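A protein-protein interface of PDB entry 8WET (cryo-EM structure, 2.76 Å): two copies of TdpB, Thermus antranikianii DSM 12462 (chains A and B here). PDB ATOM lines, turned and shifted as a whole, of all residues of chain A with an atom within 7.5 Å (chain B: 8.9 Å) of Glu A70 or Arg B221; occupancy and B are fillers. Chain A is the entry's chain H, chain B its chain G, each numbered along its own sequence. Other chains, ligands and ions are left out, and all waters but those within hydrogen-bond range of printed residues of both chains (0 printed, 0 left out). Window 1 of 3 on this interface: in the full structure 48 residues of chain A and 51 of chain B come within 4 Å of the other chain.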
ATOM      1  N   ARG A  67     -13.082  10.893  16.245  1.00  0.00           N
ATOM      2  CA  ARG A  67     -11.687  10.927  15.832  1.00  0.00           C
ATOM      3  C   ARG A  67     -10.786  11.634  16.837  1.00  0.00           C
ATOM      4  O   ARG A  67      -9.686  12.059  16.463  1.00  0.00           O
ATOM      5  CB  ARG A  67     -11.565  11.599  14.461  1.00  0.00           C
ATOM      6  CG  ARG A  67     -12.474  11.009  13.392  1.00  0.00           C
ATOM      7  CD  ARG A  67     -11.740   9.987  12.537  1.00  0.00           C
ATOM      8  NE  ARG A  67     -11.403   8.781  13.285  1.00  0.00           N
ATOM      9  CZ  ARG A  67     -12.252   7.795  13.543  1.00  0.00           C
ATOM     10  NH1 ARG A  67     -13.505   7.834  13.120  1.00  0.00           N
ATOM     11  NH2 ARG A  67     -11.833   6.745  14.242  1.00  0.00           N
ATOM     12  N   ALA A  68     -11.229  11.765  18.089  1.00  0.00           N
ATOM     13  CA  ALA A  68     -10.484  12.472  19.126  1.00  0.00           C
ATOM     14  C   ALA A  68     -10.113  13.874  18.661  1.00  0.00           C
ATOM     15  O   ALA A  68     -10.939  14.575  18.069  1.00  0.00           O
ATOM     16  CB  ALA A  68      -9.231  11.688  19.526  1.00  0.00           C
ATOM     17  N   PHE A  69      -8.874  14.293  18.923  1.00  0.00           N
ATOM     18  CA  PHE A  69      -8.385  15.589  18.481  1.00  0.00           C
ATOM     19  C   PHE A  69      -7.099  15.509  17.671  1.00  0.00           C
ATOM     20  O   PHE A  69      -6.677  16.531  17.116  1.00  0.00           O
ATOM     21  CB  PHE A  69      -8.150  16.519  19.683  1.00  0.00           C
ATOM     22  CG  PHE A  69      -9.195  16.408  20.760  1.00  0.00           C
ATOM     23  CD1 PHE A  69     -10.541  16.545  20.462  1.00  0.00           C
ATOM     24  CD2 PHE A  69      -8.828  16.165  22.073  1.00  0.00           C
ATOM     25  CE1 PHE A  69     -11.498  16.438  21.453  1.00  0.00           C
ATOM     26  CE2 PHE A  69      -9.781  16.059  23.067  1.00  0.00           C
ATOM     27  CZ  PHE A  69     -11.118  16.197  22.757  1.00  0.00           C
ATOM     28  N   GLU A  70      -6.466  14.337  17.587  1.00  0.00           N
ATOM     29  CA  GLU A  70      -5.165  14.235  16.933  1.00  0.00           C
ATOM     30  C   GLU A  70      -5.276  14.445  15.426  1.00  0.00           C
ATOM     31  O   GLU A  70      -4.521  15.230  14.843  1.00  0.00           O
ATOM     32  CB  GLU A  70      -4.530  12.880  17.247  1.00  0.00           C
ATOM     33  CG  GLU A  70      -4.297  12.640  18.730  1.00  0.00           C
ATOM     34  CD  GLU A  70      -3.293  13.608  19.325  1.00  0.00           C
ATOM     35  OE1 GLU A  70      -2.400  14.066  18.582  1.00  0.00           O
ATOM     36  OE2 GLU A  70      -3.398  13.915  20.530  1.00  0.00           O
ATOM     37  N   GLU A  71      -6.211  13.753  14.779  1.00  0.00           N
ATOM     38  CA  GLU A  71      -6.397  13.882  13.339  1.00  0.00           C
ATOM     39  C   GLU A  71      -7.403  14.962  12.966  1.00  0.00           C
ATOM     40  O   GLU A  71      -7.422  15.397  11.810  1.00  0.00           O
ATOM     41  CB  GLU A  71      -6.826  12.541  12.733  1.00  0.00           C
ATOM     42  CG  GLU A  71      -8.070  11.934  13.357  1.00  0.00           C
ATOM     43  CD  GLU A  71      -7.740  10.898  14.413  1.00  0.00           C
ATOM     44  OE1 GLU A  71      -6.596  10.903  14.915  1.00  0.00           O
ATOM     45  OE2 GLU A  71      -8.620  10.073  14.734  1.00  0.00           O
ATOM     46  N   LEU A  72      -8.229  15.402  13.904  1.00  0.00           N
ATOM     47  CA  LEU A  72      -9.147  16.508  13.681  1.00  0.00           C
ATOM     48  C   LEU A  72      -8.383  17.822  13.666  1.00  0.00           C
ATOM     49  O   LEU A  72      -7.244  17.905  14.132  1.00  0.00           O
ATOM     50  CB  LEU A  72     -10.227  16.509  14.760  1.00  0.00           C
ATOM     51  CG  LEU A  72     -11.343  15.473  14.612  1.00  0.00           C
ATOM     52  CD1 LEU A  72     -12.469  15.771  15.586  1.00  0.00           C
ATOM     53  CD2 LEU A  72     -11.863  15.428  13.186  1.00  0.00           C
ATOM     54  N   PRO A  73      -8.981  18.887  13.119  1.00  0.00           N
ATOM     55  CA  PRO A  73      -8.294  20.190  13.102  1.00  0.00           C
ATOM     56  C   PRO A  73      -7.959  20.743  14.479  1.00  0.00           C
ATOM     57  O   PRO A  73      -7.322  21.802  14.552  1.00  0.00           O
ATOM     58  CB  PRO A  73      -9.287  21.107  12.368  1.00  0.00           C
ATOM     59  CG  PRO A  73     -10.596  20.375  12.393  1.00  0.00           C
ATOM     60  CD  PRO A  73     -10.239  18.928  12.355  1.00  0.00           C
ATOM     61  N   LEU A  74      -8.378  20.081  15.559  1.00  0.00           N
ATOM     62  CA  LEU A  74      -8.122  20.446  16.951  1.00  0.00           C
ATOM     63  C   LEU A  74      -8.880  21.705  17.360  1.00  0.00           C
ATOM     64  O   LEU A  74      -8.859  22.071  18.540  1.00  0.00           O
ATOM     65  CB  LEU A  74      -6.616  20.609  17.233  1.00  0.00           C
ATOM     66  CG  LEU A  74      -6.045  20.723  18.650  1.00  0.00           C
ATOM     67  CD1 LEU A  74      -4.732  19.969  18.730  1.00  0.00           C
ATOM     68  CD2 LEU A  74      -5.821  22.176  19.037  1.00  0.00           C
ATOM     69  N   ARG A 151      -9.771  16.324  27.111  1.00  0.00           N
ATOM     70  CA  ARG A 151     -10.320  14.979  26.977  1.00  0.00           C
ATOM     71  C   ARG A 151     -11.363  14.708  28.051  1.00  0.00           C
ATOM     72  O   ARG A 151     -12.414  14.117  27.774  1.00  0.00           O
ATOM     73  CB  ARG A 151      -9.201  13.938  27.050  1.00  0.00           C
ATOM     74  CG  ARG A 151      -8.712  13.436  25.702  1.00  0.00           C
ATOM     75  CD  ARG A 151      -7.571  14.284  25.165  1.00  0.00           C
ATOM     76  NE  ARG A 151      -7.129  13.825  23.854  1.00  0.00           N
ATOM     77  CZ  ARG A 151      -6.159  14.392  23.148  1.00  0.00           C
ATOM     78  NH1 ARG A 151      -5.495  15.441  23.603  1.00  0.00           N
ATOM     79  NH2 ARG A 151      -5.848  13.891  21.957  1.00  0.00           N
ATOM     80  N   ASP A 372       0.732  18.652  10.321  1.00  0.00           N
ATOM     81  CA  ASP A 372      -0.491  18.739  11.119  1.00  0.00           C
ATOM     82  C   ASP A 372      -1.331  19.962  10.763  1.00  0.00           C
ATOM     83  O   ASP A 372      -1.412  20.914  11.538  1.00  0.00           O
ATOM     84  CB  ASP A 372      -0.154  18.753  12.611  1.00  0.00           C
ATOM     85  CG  ASP A 372       0.026  17.359  13.181  1.00  0.00           C
ATOM     86  OD1 ASP A 372      -0.497  16.398  12.580  1.00  0.00           O
ATOM     87  OD2 ASP A 372       0.690  17.225  14.230  1.00  0.00           O
ATOM     88  N   THR B 217      14.880  11.580  22.340  1.00  0.00           N
ATOM     89  CA  THR B 217      13.577  11.104  21.904  1.00  0.00           C
ATOM     90  C   THR B 217      13.426  11.092  20.391  1.00  0.00           C
ATOM     91  O   THR B 217      12.445  10.531  19.891  1.00  0.00           O
ATOM     92  CB  THR B 217      12.450  11.953  22.514  1.00  0.00           C
ATOM     93  OG1 THR B 217      11.187  11.327  22.257  1.00  0.00           O
ATOM     94  CG2 THR B 217      12.441  13.344  21.913  1.00  0.00           C
ATOM     95  N   LYS B 218      14.356  11.706  19.656  1.00  0.00           N
ATOM     96  CA  LYS B 218      14.413  11.640  18.200  1.00  0.00           C
ATOM     97  C   LYS B 218      13.158  12.213  17.551  1.00  0.00           C
ATOM     98  O   LYS B 218      13.174  13.337  17.042  1.00  0.00           O
ATOM     99  CB  LYS B 218      14.640  10.196  17.741  1.00  0.00           C
ATOM    100  CG  LYS B 218      14.843  10.040  16.242  1.00  0.00           C
ATOM    101  CD  LYS B 218      13.699   9.263  15.614  1.00  0.00           C
ATOM    102  CE  LYS B 218      13.596   9.534  14.124  1.00  0.00           C
ATOM    103  NZ  LYS B 218      12.444   8.814  13.513  1.00  0.00           N
ATOM    104  N   ARG B 219      12.070  11.443  17.561  1.00  0.00           N
ATOM    105  CA  ARG B 219      10.849  11.820  16.863  1.00  0.00           C
ATOM    106  C   ARG B 219       9.772  12.391  17.775  1.00  0.00           C
ATOM    107  O   ARG B 219       8.850  13.044  17.274  1.00  0.00           O
ATOM    108  CB  ARG B 219      10.274  10.612  16.112  1.00  0.00           C
ATOM    109  CG  ARG B 219       9.491   9.640  16.990  1.00  0.00           C
ATOM    110  CD  ARG B 219      10.414   8.763  17.823  1.00  0.00           C
ATOM    111  NE  ARG B 219       9.676   7.803  18.635  1.00  0.00           N
ATOM    112  CZ  ARG B 219       9.225   8.048  19.857  1.00  0.00           C
ATOM    113  NH1 ARG B 219       9.421   9.217  20.445  1.00  0.00           N
ATOM    114  NH2 ARG B 219       8.562   7.096  20.507  1.00  0.00           N
ATOM    115  N   SER B 220       9.870  12.168  19.087  1.00  0.00           N
ATOM    116  CA  SER B 220       8.821  12.545  20.031  1.00  0.00           C
ATOM    117  C   SER B 220       7.485  11.958  19.594  1.00  0.00           C
ATOM    118  O   SER B 220       7.354  10.737  19.455  1.00  0.00           O
ATOM    119  CB  SER B 220       8.730  14.067  20.168  1.00  0.00           C
ATOM    120  OG  SER B 220       7.565  14.447  20.879  1.00  0.00           O
ATOM    121  N   ARG B 221       6.490  12.811  19.375  1.00  0.00           N
ATOM    122  CA  ARG B 221       5.186  12.369  18.896  1.00  0.00           C
ATOM    123  C   ARG B 221       4.514  13.537  18.185  1.00  0.00           C
ATOM    124  O   ARG B 221       5.026  14.660  18.173  1.00  0.00           O
ATOM    125  CB  ARG B 221       4.321  11.833  20.039  1.00  0.00           C
ATOM    126  CG  ARG B 221       3.386  10.708  19.625  1.00  0.00           C
ATOM    127  CD  ARG B 221       2.412  10.359  20.736  1.00  0.00           C
ATOM    128  NE  ARG B 221       1.359   9.467  20.269  1.00  0.00           N
ATOM    129  CZ  ARG B 221       0.273   9.865  19.620  1.00  0.00           C
ATOM    130  NH1 ARG B 221       0.063  11.142  19.341  1.00  0.00           N
ATOM    131  NH2 ARG B 221      -0.625   8.959  19.241  1.00  0.00           N
ATOM    132  N   LEU B 222       3.358  13.255  17.580  1.00  0.00           N
ATOM    133  CA  LEU B 222       2.634  14.286  16.842  1.00  0.00           C
ATOM    134  C   LEU B 222       2.193  15.414  17.765  1.00  0.00           C
ATOM    135  O   LEU B 222       2.468  16.592  17.503  1.00  0.00           O
ATOM    136  CB  LEU B 222       1.429  13.671  16.129  1.00  0.00           C
ATOM    137  CG  LEU B 222       1.691  12.950  14.803  1.00  0.00           C
ATOM    138  CD1 LEU B 222       2.158  11.521  15.040  1.00  0.00           C
ATOM    139  CD2 LEU B 222       0.450  12.972  13.925  1.00  0.00           C
ATOM    140  N   LEU B 223       1.512  15.075  18.856  1.00  0.00           N
ATOM    141  CA  LEU B 223       1.056  16.053  19.838  1.00  0.00           C
ATOM    142  C   LEU B 223       1.495  15.655  21.238  1.00  0.00           C
ATOM    143  O   LEU B 223       0.728  15.752  22.201  1.00  0.00           O
ATOM    144  CB  LEU B 223      -0.459  16.236  19.784  1.00  0.00           C
ATOM    145  CG  LEU B 223      -1.036  17.285  18.826  1.00  0.00           C
ATOM    146  CD1 LEU B 223      -0.500  18.673  19.165  1.00  0.00           C
ATOM    147  CD2 LEU B 223      -0.788  16.944  17.361  1.00  0.00           C
ATOM    148  N   ALA B 224       2.738  15.186  21.371  1.00  0.00           N
ATOM    149  CA  ALA B 224       3.302  14.977  22.700  1.00  0.00           C
ATOM    150  C   ALA B 224       3.403  16.293  23.455  1.00  0.00           C
ATOM    151  O   ALA B 224       3.250  16.332  24.682  1.00  0.00           O
ATOM    152  CB  ALA B 224       4.674  14.311  22.596  1.00  0.00           C
ATOM    153  N   GLU B 225       3.653  17.379  22.737  1.00  0.00           N
ATOM    154  CA  GLU B 225       3.724  18.710  23.307  1.00  0.00           C
ATOM    155  C   GLU B 225       2.399  19.427  23.042  1.00  0.00           C
ATOM    156  O   GLU B 225       1.443  18.842  22.524  1.00  0.00           O
ATOM    157  CB  GLU B 225       4.919  19.462  22.720  1.00  0.00           C
ATOM    158  CG  GLU B 225       6.266  18.834  23.052  1.00  0.00           C
ATOM    159  CD  GLU B 225       6.580  18.853  24.534  1.00  0.00           C
ATOM    160  OE1 GLU B 225       6.140  19.789  25.227  1.00  0.00           O
ATOM    161  OE2 GLU B 225       7.269  17.926  25.006  1.00  0.00           O
ATOM    162  N   GLY B 226       2.333  20.708  23.395  1.00  0.00           N
ATOM    163  CA  GLY B 226       1.130  21.478  23.150  1.00  0.00           C
ATOM    164  C   GLY B 226       1.164  22.168  21.803  1.00  0.00           C
ATOM    165  O   GLY B 226       1.111  21.507  20.762  1.00  0.00           O
ATOM    166  N   THR B 228       3.808  23.764  20.919  1.00  0.00           N
ATOM    167  CA  THR B 228       5.215  23.760  20.536  1.00  0.00           C
ATOM    168  C   THR B 228       5.477  22.830  19.360  1.00  0.00           C
ATOM    169  O   THR B 228       6.347  23.115  18.530  1.00  0.00           O
ATOM    170  CB  THR B 228       6.082  23.360  21.731  1.00  0.00           C
ATOM    171  OG1 THR B 228       5.623  24.042  22.904  1.00  0.00           O
ATOM    172  CG2 THR B 228       7.536  23.724  21.481  1.00  0.00           C
ATOM    173  N   SER B 229       4.738  21.720  19.265  1.00  0.00           N
ATOM    174  CA  SER B 229       4.948  20.785  18.165  1.00  0.00           C
ATOM    175  C   SER B 229       4.667  21.432  16.816  1.00  0.00           C
ATOM    176  O   SER B 229       5.319  21.097  15.820  1.00  0.00           O
ATOM    177  CB  SER B 229       4.074  19.546  18.351  1.00  0.00           C
ATOM    178  OG  SER B 229       4.575  18.717  19.386  1.00  0.00           O
ATOM    179  N   LEU B 230       3.703  22.353  16.759  1.00  0.00           N
ATOM    180  CA  LEU B 230       3.422  23.051  15.509  1.00  0.00           C
ATOM    181  C   LEU B 230       4.589  23.944  15.104  1.00  0.00           C
ATOM    182  O   LEU B 230       5.069  23.876  13.967  1.00  0.00           O
ATOM    183  CB  LEU B 230       2.138  23.871  15.646  1.00  0.00           C
ATOM    184  CG  LEU B 230       0.823  23.090  15.705  1.00  0.00           C
ATOM    185  CD1 LEU B 230      -0.340  24.022  16.013  1.00  0.00           C
ATOM    186  CD2 LEU B 230       0.581  22.341  14.404  1.00  0.00           C
ATOM    187  N   MET B 232       7.705  23.907  16.242  1.00  0.00           N
ATOM    188  CA  MET B 232       8.913  23.113  16.037  1.00  0.00           C
ATOM    189  C   MET B 232       8.918  22.467  14.658  1.00  0.00           C
ATOM    190  O   MET B 232       9.969  22.369  14.015  1.00  0.00           O
ATOM    191  CB  MET B 232       9.034  22.044  17.123  1.00  0.00           C
ATOM    192  CG  MET B 232       9.515  22.563  18.465  1.00  0.00           C
ATOM    193  SD  MET B 232       9.560  21.267  19.715  1.00  0.00           S
ATOM    194  CE  MET B 232      10.894  20.248  19.092  1.00  0.00           C
ATOM    195  N   ALA B 233       7.751  22.021  14.190  1.00  0.00           N
ATOM    196  CA  ALA B 233       7.678  21.339  12.902  1.00  0.00           C
ATOM    197  C   ALA B 233       8.091  22.258  11.758  1.00  0.00           C
ATOM    198  O   ALA B 233       8.846  21.849  10.867  1.00  0.00           O
ATOM    199  CB  ALA B 233       6.265  20.804  12.676  1.00  0.00           C
ATOM    200  N   GLU B 259       0.296  20.506  29.139  1.00  0.00           N
ATOM    201  CA  GLU B 259       0.098  19.060  29.110  1.00  0.00           C
ATOM    202  C   GLU B 259      -0.836  18.583  30.215  1.00  0.00           C
ATOM    203  O   GLU B 259      -1.333  17.457  30.151  1.00  0.00           O
ATOM    204  CB  GLU B 259       1.440  18.326  29.208  1.00  0.00           C
ATOM    205  CG  GLU B 259       2.330  18.500  27.988  1.00  0.00           C
ATOM    206  CD  GLU B 259       1.540  18.554  26.695  1.00  0.00           C
ATOM    207  OE1 GLU B 259       0.895  17.550  26.325  1.00  0.00           O
ATOM    208  OE2 GLU B 259       1.556  19.624  26.053  1.00  0.00           O
ATOM    209  N   TRP B 262      -4.230  19.176  28.255  1.00  0.00           N
ATOM    210  CA  TRP B 262      -4.328  18.379  27.037  1.00  0.00           C
ATOM    211  C   TRP B 262      -3.910  16.930  27.216  1.00  0.00           C
ATOM    212  O   TRP B 262      -4.634  16.041  26.761  1.00  0.00           O
ATOM    213  CB  TRP B 262      -3.560  19.053  25.873  1.00  0.00           C
ATOM    214  CG  TRP B 262      -4.211  20.339  25.347  1.00  0.00           C
ATOM    215  CD1 TRP B 262      -5.125  20.399  24.343  1.00  0.00           C
ATOM    216  CD2 TRP B 262      -4.076  21.682  25.851  1.00  0.00           C
ATOM    217  NE1 TRP B 262      -5.523  21.692  24.133  1.00  0.00           N
ATOM    218  CE2 TRP B 262      -4.905  22.504  25.052  1.00  0.00           C
ATOM    219  CE3 TRP B 262      -3.324  22.270  26.874  1.00  0.00           C
ATOM    220  CZ2 TRP B 262      -4.999  23.879  25.249  1.00  0.00           C
ATOM    221  CZ3 TRP B 262      -3.430  23.630  27.062  1.00  0.00           C
ATOM    222  CH2 TRP B 262      -4.254  24.416  26.261  1.00  0.00           C
ATOM    223  N   ASN B 263      -2.801  16.647  27.884  1.00  0.00           N
ATOM    224  CA  ASN B 263      -2.366  15.260  27.971  1.00  0.00           C
ATOM    225  C   ASN B 263      -2.967  14.583  29.204  1.00  0.00           C
ATOM    226  O   ASN B 263      -3.852  15.122  29.874  1.00  0.00           O
ATOM    227  CB  ASN B 263      -0.842  15.170  27.957  1.00  0.00           C
ATOM    228  CG  ASN B 263      -0.342  14.062  27.053  1.00  0.00           C
ATOM    229  OD1 ASN B 263      -0.983  13.739  26.053  1.00  0.00           O
ATOM    230  ND2 ASN B 263       0.776  13.444  27.419  1.00  0.00           N
ATOM    231  N   ARG B 275      16.619  21.605  26.719  1.00  0.00           N
ATOM    232  CA  ARG B 275      16.252  20.851  25.529  1.00  0.00           C
ATOM    233  C   ARG B 275      17.012  21.382  24.319  1.00  0.00           C
ATOM    234  O   ARG B 275      17.124  22.596  24.128  1.00  0.00           O
ATOM    235  CB  ARG B 275      14.745  20.926  25.269  1.00  0.00           C
ATOM    236  CG  ARG B 275      14.301  20.212  24.003  1.00  0.00           C
ATOM    237  CD  ARG B 275      12.820  19.875  24.033  1.00  0.00           C
ATOM    238  NE  ARG B 275      12.534  18.748  24.912  1.00  0.00           N
ATOM    239  CZ  ARG B 275      11.327  18.233  25.100  1.00  0.00           C
ATOM    240  NH1 ARG B 275      10.265  18.719  24.481  1.00  0.00           N
ATOM    241  NH2 ARG B 275      11.184  17.202  25.928  1.00  0.00           N
ATOM    242  N   GLN B 288       9.698  16.924   8.282  1.00  0.00           N
ATOM    243  CA  GLN B 288      10.057  16.686   9.676  1.00  0.00           C
ATOM    244  C   GLN B 288      11.015  15.508   9.844  1.00  0.00           C
ATOM    245  O   GLN B 288      11.311  15.112  10.976  1.00  0.00           O
ATOM    246  CB  GLN B 288       8.774  16.488  10.495  1.00  0.00           C
ATOM    247  CG  GLN B 288       8.935  16.470  12.010  1.00  0.00           C
ATOM    248  CD  GLN B 288       7.608  16.364  12.734  1.00  0.00           C
ATOM    249  OE1 GLN B 288       6.553  16.271  12.108  1.00  0.00           O
ATOM    250  NE2 GLN B 288       7.654  16.382  14.060  1.00  0.00           N
ATOM    251  N   ILE B 293      15.595  15.271  18.995  1.00  0.00           N
ATOM    252  CA  ILE B 293      15.340  16.073  20.185  1.00  0.00           C
ATOM    253  C   ILE B 293      15.927  15.336  21.378  1.00  0.00           C
ATOM    254  O   ILE B 293      15.577  14.176  21.632  1.00  0.00           O
ATOM    255  CB  ILE B 293      13.841  16.344  20.393  1.00  0.00           C
ATOM    256  CG1 ILE B 293      13.266  17.175  19.241  1.00  0.00           C
ATOM    257  CG2 ILE B 293      13.605  17.043  21.722  1.00  0.00           C
ATOM    258  CD1 ILE B 293      12.739  16.360  18.080  1.00  0.00           C
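NH1 of Arg B221 lies within salt-bridge range of OE1 of Glu A70 (3.9 Å). NH1 of Arg A151 sits at hydrogen-bond distance from O of Trp B262.
The guanidinium group (NH2) of Arg A151 is in salt-bridge range of the side-chain carboxylate (OE2) of Glu A70 (2.8 Å).
Among the printed residues, pairs that only touch across the chains: Glu A70 with Leu B223 (3.1 Å), Asp A372 with Leu B223 (3.5 Å), Asp A372 with Leu B230 (3.8 Å) and Asp A372 with Leu B222 (3.8 Å).
Of chain B, only Arg B221 (3.9 Å) and Leu B223 (3.1 Å) come within 4 Å of Glu A70. Arg B221 touches just one residue of chain A: Glu A70 (3.9 Å). Of the printed residues of chain A, Leu B222 touches Asp A372 (3.8 Å). Printed residues of chain B within 4 Å of Arg A151: Trp B262. Printed residues of chain A within 4 Å of Trp B262: Arg A151 (3.3 Å).
Of the 21 printed residues of chain B, 5 touch a printed residue of chain A. Hydrophobic or aromatic side chains of chain B that line the printed part of chain A: Leu B222, Leu B223 and Leu B230. Among the printed residues, Asp or Glu carboxylates within 4 Å of a Lys or Arg side-chain nitrogen of the other chain: Glu A70 with Arg B221 (3.9 Å).
No position is printed for both chains. Of the 6 pairs that touch across the chains among the printed residues, none has its exchanged pair printed and touching as well.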
